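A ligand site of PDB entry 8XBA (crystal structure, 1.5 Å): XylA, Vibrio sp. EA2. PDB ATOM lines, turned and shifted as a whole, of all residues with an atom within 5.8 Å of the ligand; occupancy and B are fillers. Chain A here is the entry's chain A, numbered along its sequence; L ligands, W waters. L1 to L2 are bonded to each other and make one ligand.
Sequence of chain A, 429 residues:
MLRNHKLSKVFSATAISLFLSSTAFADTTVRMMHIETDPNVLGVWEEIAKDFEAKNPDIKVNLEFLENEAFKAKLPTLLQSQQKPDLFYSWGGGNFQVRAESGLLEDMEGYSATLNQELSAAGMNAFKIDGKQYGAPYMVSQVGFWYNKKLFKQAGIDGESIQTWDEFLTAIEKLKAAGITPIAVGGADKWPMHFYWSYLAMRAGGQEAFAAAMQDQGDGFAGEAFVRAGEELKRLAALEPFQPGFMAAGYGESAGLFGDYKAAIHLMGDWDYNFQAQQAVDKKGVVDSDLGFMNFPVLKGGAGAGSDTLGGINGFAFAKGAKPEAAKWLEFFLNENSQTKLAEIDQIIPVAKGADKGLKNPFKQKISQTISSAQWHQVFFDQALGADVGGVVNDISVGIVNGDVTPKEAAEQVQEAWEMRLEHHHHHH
The side-chain carboxylate (OD1) of Asp 382 sits at hydrogen-bond distance from an oxygen (O3) of LG2 L2 (2.7 Å).
O1 of LG2 L2 sits at hydrogen-bond distance from ND2 of Asn 68 (2.9 Å).
An oxygen (O1) of LG2 L2 sits at hydrogen-bond distance from the side-chain amino group of Lys 72.
The side-chain hydroxyl (OH) of Tyr 89 sits at hydrogen-bond distance from an oxygen (O3) of LIG L1.
NE2 of Gln 383 is in hydrogen-bond range of O2 of LG2 L2, at 3.0 Å.
An oxygen (O4) of LIG L1 sits at hydrogen-bond distance from the indole nitrogen of Trp 91 (3.2 Å).
The indole nitrogen (NE1) of Trp 271 sits at hydrogen-bond distance from an oxygen (O5) of LIG L1.
The side-chain amide nitrogen (ND2) of Asn 314 is in hydrogen-bond range of an oxygen (O3) of LIG L1, at 3.3 Å.
The side-chain carboxylate (OD2) of Asp 382 is in hydrogen-bond range of the side-chain amide nitrogen (ND2) of Asn 394, at 3.1 Å.
The side-chain carboxylate (OE1) of Glu 69 lies close to the side-chain amide oxygen (OD1) of Asn 68 (3.4 Å).
The side-chain amino group (NZ) of Lys 72 is in salt-bridge range of the side-chain carboxylate (OE1) of Glu 69 (2.8 Å).
The side-chain amide nitrogen (ND2) of Asn 314 lies within hydrogen-bond range of the side-chain hydroxyl (OH) of Tyr 89 (2.7 Å).
O of Trp 191 sits at hydrogen-bond distance from ND1 of His 194, at 2.7 Å.
The indole nitrogen of Trp 271 is in hydrogen-bond range of the side-chain hydroxyl of Tyr 251 (3.0 Å).
The indole nitrogen (NE1) of Trp 271 is in hydrogen-bond range of the side-chain sulfur (SD) of Met 268 (3.5 Å).
The indole nitrogen of Trp 191 sits at hydrogen-bond distance from the side-chain carboxylate of Glu 69.
Ile 35 touches the ligand.
Trp 191 touches the ligand.
CE1 of His 194 touches O3 of LG2 L2, at 3.2 Å.
CE1 of Phe 195 touches O3 of LG2 L2 (3.7 Å).
CE2 of Tyr 251 touches O5 of LIG L1 (3.5 Å).
CB of Phe 380 touches O3 of LG2 L2, at 3.6 Å.
Hydrophobic or aromatic side chains within 4 Å of the ligand: Ile 35, Tyr 89, Trp 91, Trp 191, His 194, Phe 195, Tyr 251, Trp 271 and Phe 380.
Within 4 Å of the ligand: Ile 35, Asn 68, Lys 72, Tyr 89, Trp 91, Trp 191, His 194, Phe 195, Tyr 251, Trp 271, Asn 314, Phe 380, Asp 382 and Gln 383.
Water W4 lies within hydrogen-bond range of O3 of LIG L1 (2.7 Å), ND2 of Asn 314 (2.9 Å) and NE1 of Trp 91 (3.2 Å).
Water W1 lies within hydrogen-bond range of the backbone carbonyl oxygen (O) of Ile 35 (2.8 Å) and an oxygen (O2) of LIG L1 (2.9 Å).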
ATOM      1  N   ILE A  35     -17.722   8.491   6.162  1.00  0.00           N
ATOM      2  CA  ILE A  35     -17.705   9.843   5.616  1.00  0.00           C
ATOM      3  C   ILE A  35     -17.556   9.839   4.101  1.00  0.00           C
ATOM      4  O   ILE A  35     -17.185  10.836   3.503  1.00  0.00           O
ATOM      5  CB  ILE A  35     -16.611  10.703   6.284  1.00  0.00           C
ATOM      6  CG1 ILE A  35     -15.219  10.146   5.978  1.00  0.00           C
ATOM      7  CG2 ILE A  35     -16.824  10.773   7.808  1.00  0.00           C
ATOM      8  CD1 ILE A  35     -14.119  11.172   6.171  1.00  0.00           C
ATOM      9  N   GLU A  36     -17.849   8.710   3.462  1.00  0.00           N
ATOM     10  CA  GLU A  36     -17.648   8.562   2.026  1.00  0.00           C
ATOM     11  C   GLU A  36     -18.789   9.172   1.209  1.00  0.00           C
ATOM     12  O   GLU A  36     -19.969   8.885   1.457  1.00  0.00           O
ATOM     13  CB  GLU A  36     -17.500   7.077   1.690  1.00  0.00           C
ATOM     14  CG  GLU A  36     -17.135   6.816   0.243  1.00  0.00           C
ATOM     15  CD  GLU A  36     -15.906   7.574  -0.192  1.00  0.00           C
ATOM     16  OE1 GLU A  36     -16.024   8.578  -0.940  1.00  0.00           O
ATOM     17  OE2 GLU A  36     -14.795   7.182   0.230  1.00  0.00           O
ATOM     18  N   ASN A  68     -17.479  14.671   6.546  1.00  0.00           N
ATOM     19  CA  ASN A  68     -16.211  14.854   7.253  1.00  0.00           C
ATOM     20  C   ASN A  68     -16.267  15.802   8.464  1.00  0.00           C
ATOM     21  O   ASN A  68     -16.055  15.392   9.604  1.00  0.00           O
ATOM     22  CB  ASN A  68     -15.167  15.313   6.234  1.00  0.00           C
ATOM     23  CG  ASN A  68     -13.777  15.543   6.833  1.00  0.00           C
ATOM     24  OD1 ASN A  68     -13.109  16.539   6.500  1.00  0.00           O
ATOM     25  ND2 ASN A  68     -13.314  14.629   7.651  1.00  0.00           N
ATOM     26  N   GLU A  69     -16.547  17.084   8.228  1.00  0.00           N
ATOM     27  CA  GLU A  69     -16.515  18.041   9.334  1.00  0.00           C
ATOM     28  C   GLU A  69     -17.626  17.780  10.347  1.00  0.00           C
ATOM     29  O   GLU A  69     -17.412  17.880  11.560  1.00  0.00           O
ATOM     30  CB  GLU A  69     -16.583  19.461   8.803  1.00  0.00           C
ATOM     31  CG  GLU A  69     -15.344  19.908   8.057  1.00  0.00           C
ATOM     32  CD  GLU A  69     -14.123  19.886   8.942  1.00  0.00           C
ATOM     33  OE1 GLU A  69     -13.116  19.299   8.537  1.00  0.00           O
ATOM     34  OE2 GLU A  69     -14.173  20.459  10.051  1.00  0.00           O
ATOM     35  N   LYS A  72     -16.658  14.676  12.509  1.00  0.00           N
ATOM     36  CA  LYS A  72     -15.685  14.930  13.565  1.00  0.00           C
ATOM     37  C   LYS A  72     -16.335  15.698  14.711  1.00  0.00           C
ATOM     38  O   LYS A  72     -16.014  15.459  15.879  1.00  0.00           O
ATOM     39  CB  LYS A  72     -14.477  15.685  13.012  1.00  0.00           C
ATOM     40  CG  LYS A  72     -13.613  14.828  12.083  1.00  0.00           C
ATOM     41  CD  LYS A  72     -12.404  15.618  11.569  1.00  0.00           C
ATOM     42  CE  LYS A  72     -12.809  16.756  10.659  1.00  0.00           C
ATOM     43  NZ  LYS A  72     -11.617  17.529  10.140  1.00  0.00           N
ATOM     44  N   TYR A  89     -15.604   5.397  11.233  1.00  0.00           N
ATOM     45  CA  TYR A  89     -14.373   5.799  10.569  1.00  0.00           C
ATOM     46  C   TYR A  89     -13.424   6.485  11.553  1.00  0.00           C
ATOM     47  O   TYR A  89     -13.848   7.257  12.412  1.00  0.00           O
ATOM     48  CB  TYR A  89     -14.717   6.799   9.469  1.00  0.00           C
ATOM     49  CG  TYR A  89     -13.623   7.141   8.478  1.00  0.00           C
ATOM     50  CD1 TYR A  89     -13.236   6.236   7.500  1.00  0.00           C
ATOM     51  CD2 TYR A  89     -13.040   8.402   8.479  1.00  0.00           C
ATOM     52  CE1 TYR A  89     -12.274   6.561   6.552  1.00  0.00           C
ATOM     53  CE2 TYR A  89     -12.073   8.748   7.544  1.00  0.00           C
ATOM     54  CZ  TYR A  89     -11.715   7.829   6.569  1.00  0.00           C
ATOM     55  OH  TYR A  89     -10.782   8.199   5.625  1.00  0.00           O
ATOM     56  N   TRP A  91      -9.156   8.059  12.083  1.00  0.00           N
ATOM     57  CA  TRP A  91      -7.821   8.416  11.638  1.00  0.00           C
ATOM     58  C   TRP A  91      -6.758   7.852  12.554  1.00  0.00           C
ATOM     59  O   TRP A  91      -5.582   8.181  12.397  1.00  0.00           O
ATOM     60  CB  TRP A  91      -7.659   9.939  11.567  1.00  0.00           C
ATOM     61  CG  TRP A  91      -8.515  10.602  10.493  1.00  0.00           C
ATOM     62  CD1 TRP A  91      -8.127  10.908   9.231  1.00  0.00           C
ATOM     63  CD2 TRP A  91      -9.895  11.012  10.605  1.00  0.00           C
ATOM     64  NE1 TRP A  91      -9.162  11.500   8.536  1.00  0.00           N
ATOM     65  CE2 TRP A  91     -10.258  11.567   9.368  1.00  0.00           C
ATOM     66  CE3 TRP A  91     -10.842  10.959  11.635  1.00  0.00           C
ATOM     67  CZ2 TRP A  91     -11.545  12.065   9.110  1.00  0.00           C
ATOM     68  CZ3 TRP A  91     -12.120  11.463  11.387  1.00  0.00           C
ATOM     69  CH2 TRP A  91     -12.461  12.012  10.134  1.00  0.00           C
ATOM     70  N   MET A 139      -7.219   2.062   4.725  1.00  0.00           N
ATOM     71  CA  MET A 139      -6.402   2.656   3.692  1.00  0.00           C
ATOM     72  C   MET A 139      -5.198   3.430   4.208  1.00  0.00           C
ATOM     73  O   MET A 139      -5.169   3.788   5.348  1.00  0.00           O
ATOM     74  CB  MET A 139      -7.241   3.598   2.791  1.00  0.00           C
ATOM     75  CG  MET A 139      -7.847   4.814   3.495  1.00  0.00           C
ATOM     76  SD  MET A 139      -6.761   6.247   3.689  1.00  0.00           S
ATOM     77  CE  MET A 139      -7.902   7.575   3.259  1.00  0.00           C
ATOM     78  N   TRP A 191      -7.976  22.487   8.169  1.00  0.00           N
ATOM     79  CA  TRP A 191      -7.032  21.386   7.960  1.00  0.00           C
ATOM     80  C   TRP A 191      -6.363  21.389   6.571  1.00  0.00           C
ATOM     81  O   TRP A 191      -5.198  20.961   6.500  1.00  0.00           O
ATOM     82  CB  TRP A 191      -7.648  20.035   8.351  1.00  0.00           C
ATOM     83  CG  TRP A 191      -8.821  19.614   7.515  1.00  0.00           C
ATOM     84  CD1 TRP A 191     -10.148  19.768   7.815  1.00  0.00           C
ATOM     85  CD2 TRP A 191      -8.776  18.977   6.220  1.00  0.00           C
ATOM     86  NE1 TRP A 191     -10.925  19.266   6.806  1.00  0.00           N
ATOM     87  CE2 TRP A 191     -10.117  18.787   5.817  1.00  0.00           C
ATOM     88  CE3 TRP A 191      -7.746  18.566   5.373  1.00  0.00           C
ATOM     89  CZ2 TRP A 191     -10.453  18.191   4.603  1.00  0.00           C
ATOM     90  CZ3 TRP A 191      -8.073  17.972   4.160  1.00  0.00           C
ATOM     91  CH2 TRP A 191      -9.417  17.787   3.788  1.00  0.00           C
ATOM     92  N   HIS A 194      -3.381  23.446   7.118  1.00  0.00           N
ATOM     93  CA  HIS A 194      -2.397  22.830   8.003  1.00  0.00           C
ATOM     94  C   HIS A 194      -1.432  21.876   7.321  1.00  0.00           C
ATOM     95  O   HIS A 194      -0.393  21.625   7.801  1.00  0.00           O
ATOM     96  CB  HIS A 194      -3.057  22.276   9.286  1.00  0.00           C
ATOM     97  CG  HIS A 194      -3.087  20.786   9.420  1.00  0.00           C
ATOM     98  ND1 HIS A 194      -3.865  19.979   8.629  1.00  0.00           N
ATOM     99  CD2 HIS A 194      -2.541  19.984  10.352  1.00  0.00           C
ATOM    100  CE1 HIS A 194      -3.748  18.738   9.033  1.00  0.00           C
ATOM    101  NE2 HIS A 194      -2.947  18.713  10.075  1.00  0.00           N
ATOM    102  N   PHE A 195      -1.852  21.370   6.181  1.00  0.00           N
ATOM    103  CA  PHE A 195      -0.938  20.568   5.393  1.00  0.00           C
ATOM    104  C   PHE A 195       0.330  21.356   5.041  1.00  0.00           C
ATOM    105  O   PHE A 195       1.429  20.782   4.995  1.00  0.00           O
ATOM    106  CB  PHE A 195      -1.609  20.103   4.104  1.00  0.00           C
ATOM    107  CG  PHE A 195      -2.682  19.052   4.279  1.00  0.00           C
ATOM    108  CD1 PHE A 195      -2.851  18.361   5.471  1.00  0.00           C
ATOM    109  CD2 PHE A 195      -3.511  18.738   3.224  1.00  0.00           C
ATOM    110  CE1 PHE A 195      -3.842  17.385   5.596  1.00  0.00           C
ATOM    111  CE2 PHE A 195      -4.492  17.767   3.336  1.00  0.00           C
ATOM    112  CZ  PHE A 195      -4.653  17.087   4.524  1.00  0.00           C
ATOM    113  N   TYR A 251     -13.492  22.275   1.817  1.00  0.00           N
ATOM    114  CA  TYR A 251     -12.764  21.352   0.946  1.00  0.00           C
ATOM    115  C   TYR A 251     -13.537  21.051  -0.337  1.00  0.00           C
ATOM    116  O   TYR A 251     -12.957  21.021  -1.422  1.00  0.00           O
ATOM    117  CB  TYR A 251     -12.406  20.079   1.738  1.00  0.00           C
ATOM    118  CG  TYR A 251     -11.825  18.945   0.901  1.00  0.00           C
ATOM    119  CD1 TYR A 251     -10.885  19.190  -0.100  1.00  0.00           C
ATOM    120  CD2 TYR A 251     -12.219  17.627   1.116  1.00  0.00           C
ATOM    121  CE1 TYR A 251     -10.367  18.154  -0.875  1.00  0.00           C
ATOM    122  CE2 TYR A 251     -11.702  16.586   0.354  1.00  0.00           C
ATOM    123  CZ  TYR A 251     -10.778  16.857  -0.639  1.00  0.00           C
ATOM    124  OH  TYR A 251     -10.260  15.816  -1.401  1.00  0.00           O
ATOM    125  N   MET A 268      -3.244  18.031  -1.288  1.00  0.00           N
ATOM    126  CA  MET A 268      -4.336  17.212  -0.771  1.00  0.00           C
ATOM    127  C   MET A 268      -3.905  15.753  -0.733  1.00  0.00           C
ATOM    128  O   MET A 268      -2.958  15.332  -1.417  1.00  0.00           O
ATOM    129  CB  MET A 268      -5.615  17.368  -1.614  1.00  0.00           C
ATOM    130  CG  MET A 268      -6.911  16.791  -1.015  1.00  0.00           C
ATOM    131  SD  MET A 268      -7.260  17.170   0.729  1.00  0.00           S
ATOM    132  CE  MET A 268      -7.240  18.956   0.683  1.00  0.00           C
ATOM    133  N   TRP A 271      -6.836  10.779  -2.084  1.00  0.00           N
ATOM    134  CA  TRP A 271      -8.274  10.659  -2.325  1.00  0.00           C
ATOM    135  C   TRP A 271      -8.830  11.806  -3.163  1.00  0.00           C
ATOM    136  O   TRP A 271      -9.979  11.706  -3.617  1.00  0.00           O
ATOM    137  CB  TRP A 271      -9.009  10.646  -0.977  1.00  0.00           C
ATOM    138  CG  TRP A 271      -8.787  11.914  -0.162  1.00  0.00           C
ATOM    139  CD1 TRP A 271      -9.406  13.125  -0.339  1.00  0.00           C
ATOM    140  CD2 TRP A 271      -7.852  12.085   0.922  1.00  0.00           C
ATOM    141  NE1 TRP A 271      -8.912  14.043   0.571  1.00  0.00           N
ATOM    142  CE2 TRP A 271      -7.992  13.423   1.365  1.00  0.00           C
ATOM    143  CE3 TRP A 271      -6.950  11.239   1.573  1.00  0.00           C
ATOM    144  CZ2 TRP A 271      -7.231  13.939   2.421  1.00  0.00           C
ATOM    145  CZ3 TRP A 271      -6.210  11.747   2.641  1.00  0.00           C
ATOM    146  CH2 TRP A 271      -6.345  13.083   3.039  1.00  0.00           C
ATOM    147  N   ASN A 314      -5.944   5.214   7.843  1.00  0.00           N
ATOM    148  CA  ASN A 314      -7.321   5.351   8.306  1.00  0.00           C
ATOM    149  C   ASN A 314      -7.970   3.982   8.376  1.00  0.00           C
ATOM    150  O   ASN A 314      -7.529   3.027   7.738  1.00  0.00           O
ATOM    151  CB  ASN A 314      -8.111   6.267   7.369  1.00  0.00           C
ATOM    152  CG  ASN A 314      -7.614   7.698   7.399  1.00  0.00           C
ATOM    153  OD1 ASN A 314      -6.609   7.999   8.051  1.00  0.00           O
ATOM    154  ND2 ASN A 314      -8.307   8.589   6.715  1.00  0.00           N
ATOM    155  N   PHE A 380      -1.211  12.909   9.840  1.00  0.00           N
ATOM    156  CA  PHE A 380      -1.635  14.309   9.860  1.00  0.00           C
ATOM    157  C   PHE A 380      -1.471  14.872  11.257  1.00  0.00           C
ATOM    158  O   PHE A 380      -1.912  14.260  12.229  1.00  0.00           O
ATOM    159  CB  PHE A 380      -3.135  14.411   9.495  1.00  0.00           C
ATOM    160  CG  PHE A 380      -3.527  13.616   8.291  1.00  0.00           C
ATOM    161  CD1 PHE A 380      -3.121  13.997   7.013  1.00  0.00           C
ATOM    162  CD2 PHE A 380      -4.294  12.462   8.439  1.00  0.00           C
ATOM    163  CE1 PHE A 380      -3.497  13.246   5.903  1.00  0.00           C
ATOM    164  CE2 PHE A 380      -4.669  11.707   7.321  1.00  0.00           C
ATOM    165  CZ  PHE A 380      -4.255  12.103   6.047  1.00  0.00           C
ATOM    166  N   ASP A 382      -2.936  17.295  12.789  1.00  0.00           N
ATOM    167  CA  ASP A 382      -4.154  17.552  13.538  1.00  0.00           C
ATOM    168  C   ASP A 382      -4.757  16.274  14.111  1.00  0.00           C
ATOM    169  O   ASP A 382      -5.426  16.317  15.138  1.00  0.00           O
ATOM    170  CB  ASP A 382      -5.159  18.408  12.747  1.00  0.00           C
ATOM    171  CG  ASP A 382      -5.900  17.638  11.652  1.00  0.00           C
ATOM    172  OD1 ASP A 382      -5.360  16.653  11.118  1.00  0.00           O
ATOM    173  OD2 ASP A 382      -7.035  18.067  11.320  1.00  0.00           O
ATOM    174  N   GLN A 383      -4.517  15.137  13.469  1.00  0.00           N
ATOM    175  CA  GLN A 383      -4.986  13.867  14.004  1.00  0.00           C
ATOM    176  C   GLN A 383      -4.002  13.262  14.987  1.00  0.00           C
ATOM    177  O   GLN A 383      -4.429  12.629  15.961  1.00  0.00           O
ATOM    178  CB  GLN A 383      -5.287  12.891  12.849  1.00  0.00           C
ATOM    179  CG  GLN A 383      -6.395  13.373  11.924  1.00  0.00           C
ATOM    180  CD  GLN A 383      -7.732  13.473  12.612  1.00  0.00           C
ATOM    181  OE1 GLN A 383      -7.977  12.783  13.605  1.00  0.00           O
ATOM    182  NE2 GLN A 383      -8.614  14.318  12.093  1.00  0.00           N
ATOM    183  N   ASN A 394      -4.561  23.643  13.447  1.00  0.00           N
ATOM    184  CA  ASN A 394      -5.419  24.101  12.361  1.00  0.00           C
ATOM    185  C   ASN A 394      -5.663  25.601  12.449  1.00  0.00           C
ATOM    186  O   ASN A 394      -5.603  26.311  11.435  1.00  0.00           O
ATOM    187  CB  ASN A 394      -6.736  23.332  12.379  1.00  0.00           C
ATOM    188  CG  ASN A 394      -6.603  21.928  11.786  1.00  0.00           C
ATOM    189  OD1 ASN A 394      -5.678  21.658  11.026  1.00  0.00           O
ATOM    190  ND2 ASN A 394      -7.515  21.035  12.133  1.00  0.00           N
HETATM  191  C1  LIG L   1     -11.837  13.004   2.620  1.00  0.00           C
HETATM  192  C2  LIG L   1     -11.062  11.829   3.200  1.00  0.00           C
HETATM  193  C3  LIG L   1     -10.812  12.058   4.684  1.00  0.00           C
HETATM  194  C4  LIG L   1     -10.116  13.394   4.885  1.00  0.00           C
HETATM  195  C5  LIG L   1     -11.028  14.477   4.320  1.00  0.00           C
HETATM  196  O1  LIG L   1     -13.151  13.087   3.194  1.00  0.00           O
HETATM  197  O2  LIG L   1     -11.815  10.618   3.046  1.00  0.00           O
HETATM  198  O3  LIG L   1     -10.072  10.974   5.229  1.00  0.00           O
HETATM  199  O4  LIG L   1      -9.983  13.624   6.301  1.00  0.00           O
HETATM  200  O5  LIG L   1     -11.178  14.225   2.913  1.00  0.00           O
HETATM  201  C1  LG2 L   2      -9.150  14.669   6.609  1.00  0.00           C
HETATM  202  C2  LG2 L   2      -9.433  15.036   8.058  1.00  0.00           C
HETATM  203  C3  LG2 L   2      -8.378  16.034   8.514  1.00  0.00           C
HETATM  204  C4  LG2 L   2      -6.985  15.433   8.292  1.00  0.00           C
HETATM  205  C5  LG2 L   2      -6.813  14.942   6.857  1.00  0.00           C
HETATM  206  O1  LG2 L   2     -10.711  15.669   8.167  1.00  0.00           O
HETATM  207  O2  LG2 L   2      -8.580  16.325   9.893  1.00  0.00           O
HETATM  208  O3  LG2 L   2      -5.963  16.425   8.524  1.00  0.00           O
HETATM  209  O4  LG2 L   2      -7.875  14.026   6.563  1.00  0.00           O
HETATM  210  O   HOH W   1     -14.602  10.394   2.433  1.00  0.00           O
HETATM  211  O   HOH W   2     -11.759   9.368   0.704  1.00  0.00           O
HETATM  212  O   HOH W   3     -15.362  15.025   2.087  1.00  0.00           O
HETATM  213  O   HOH W   4      -7.490  11.210   5.833  1.00  0.00           O
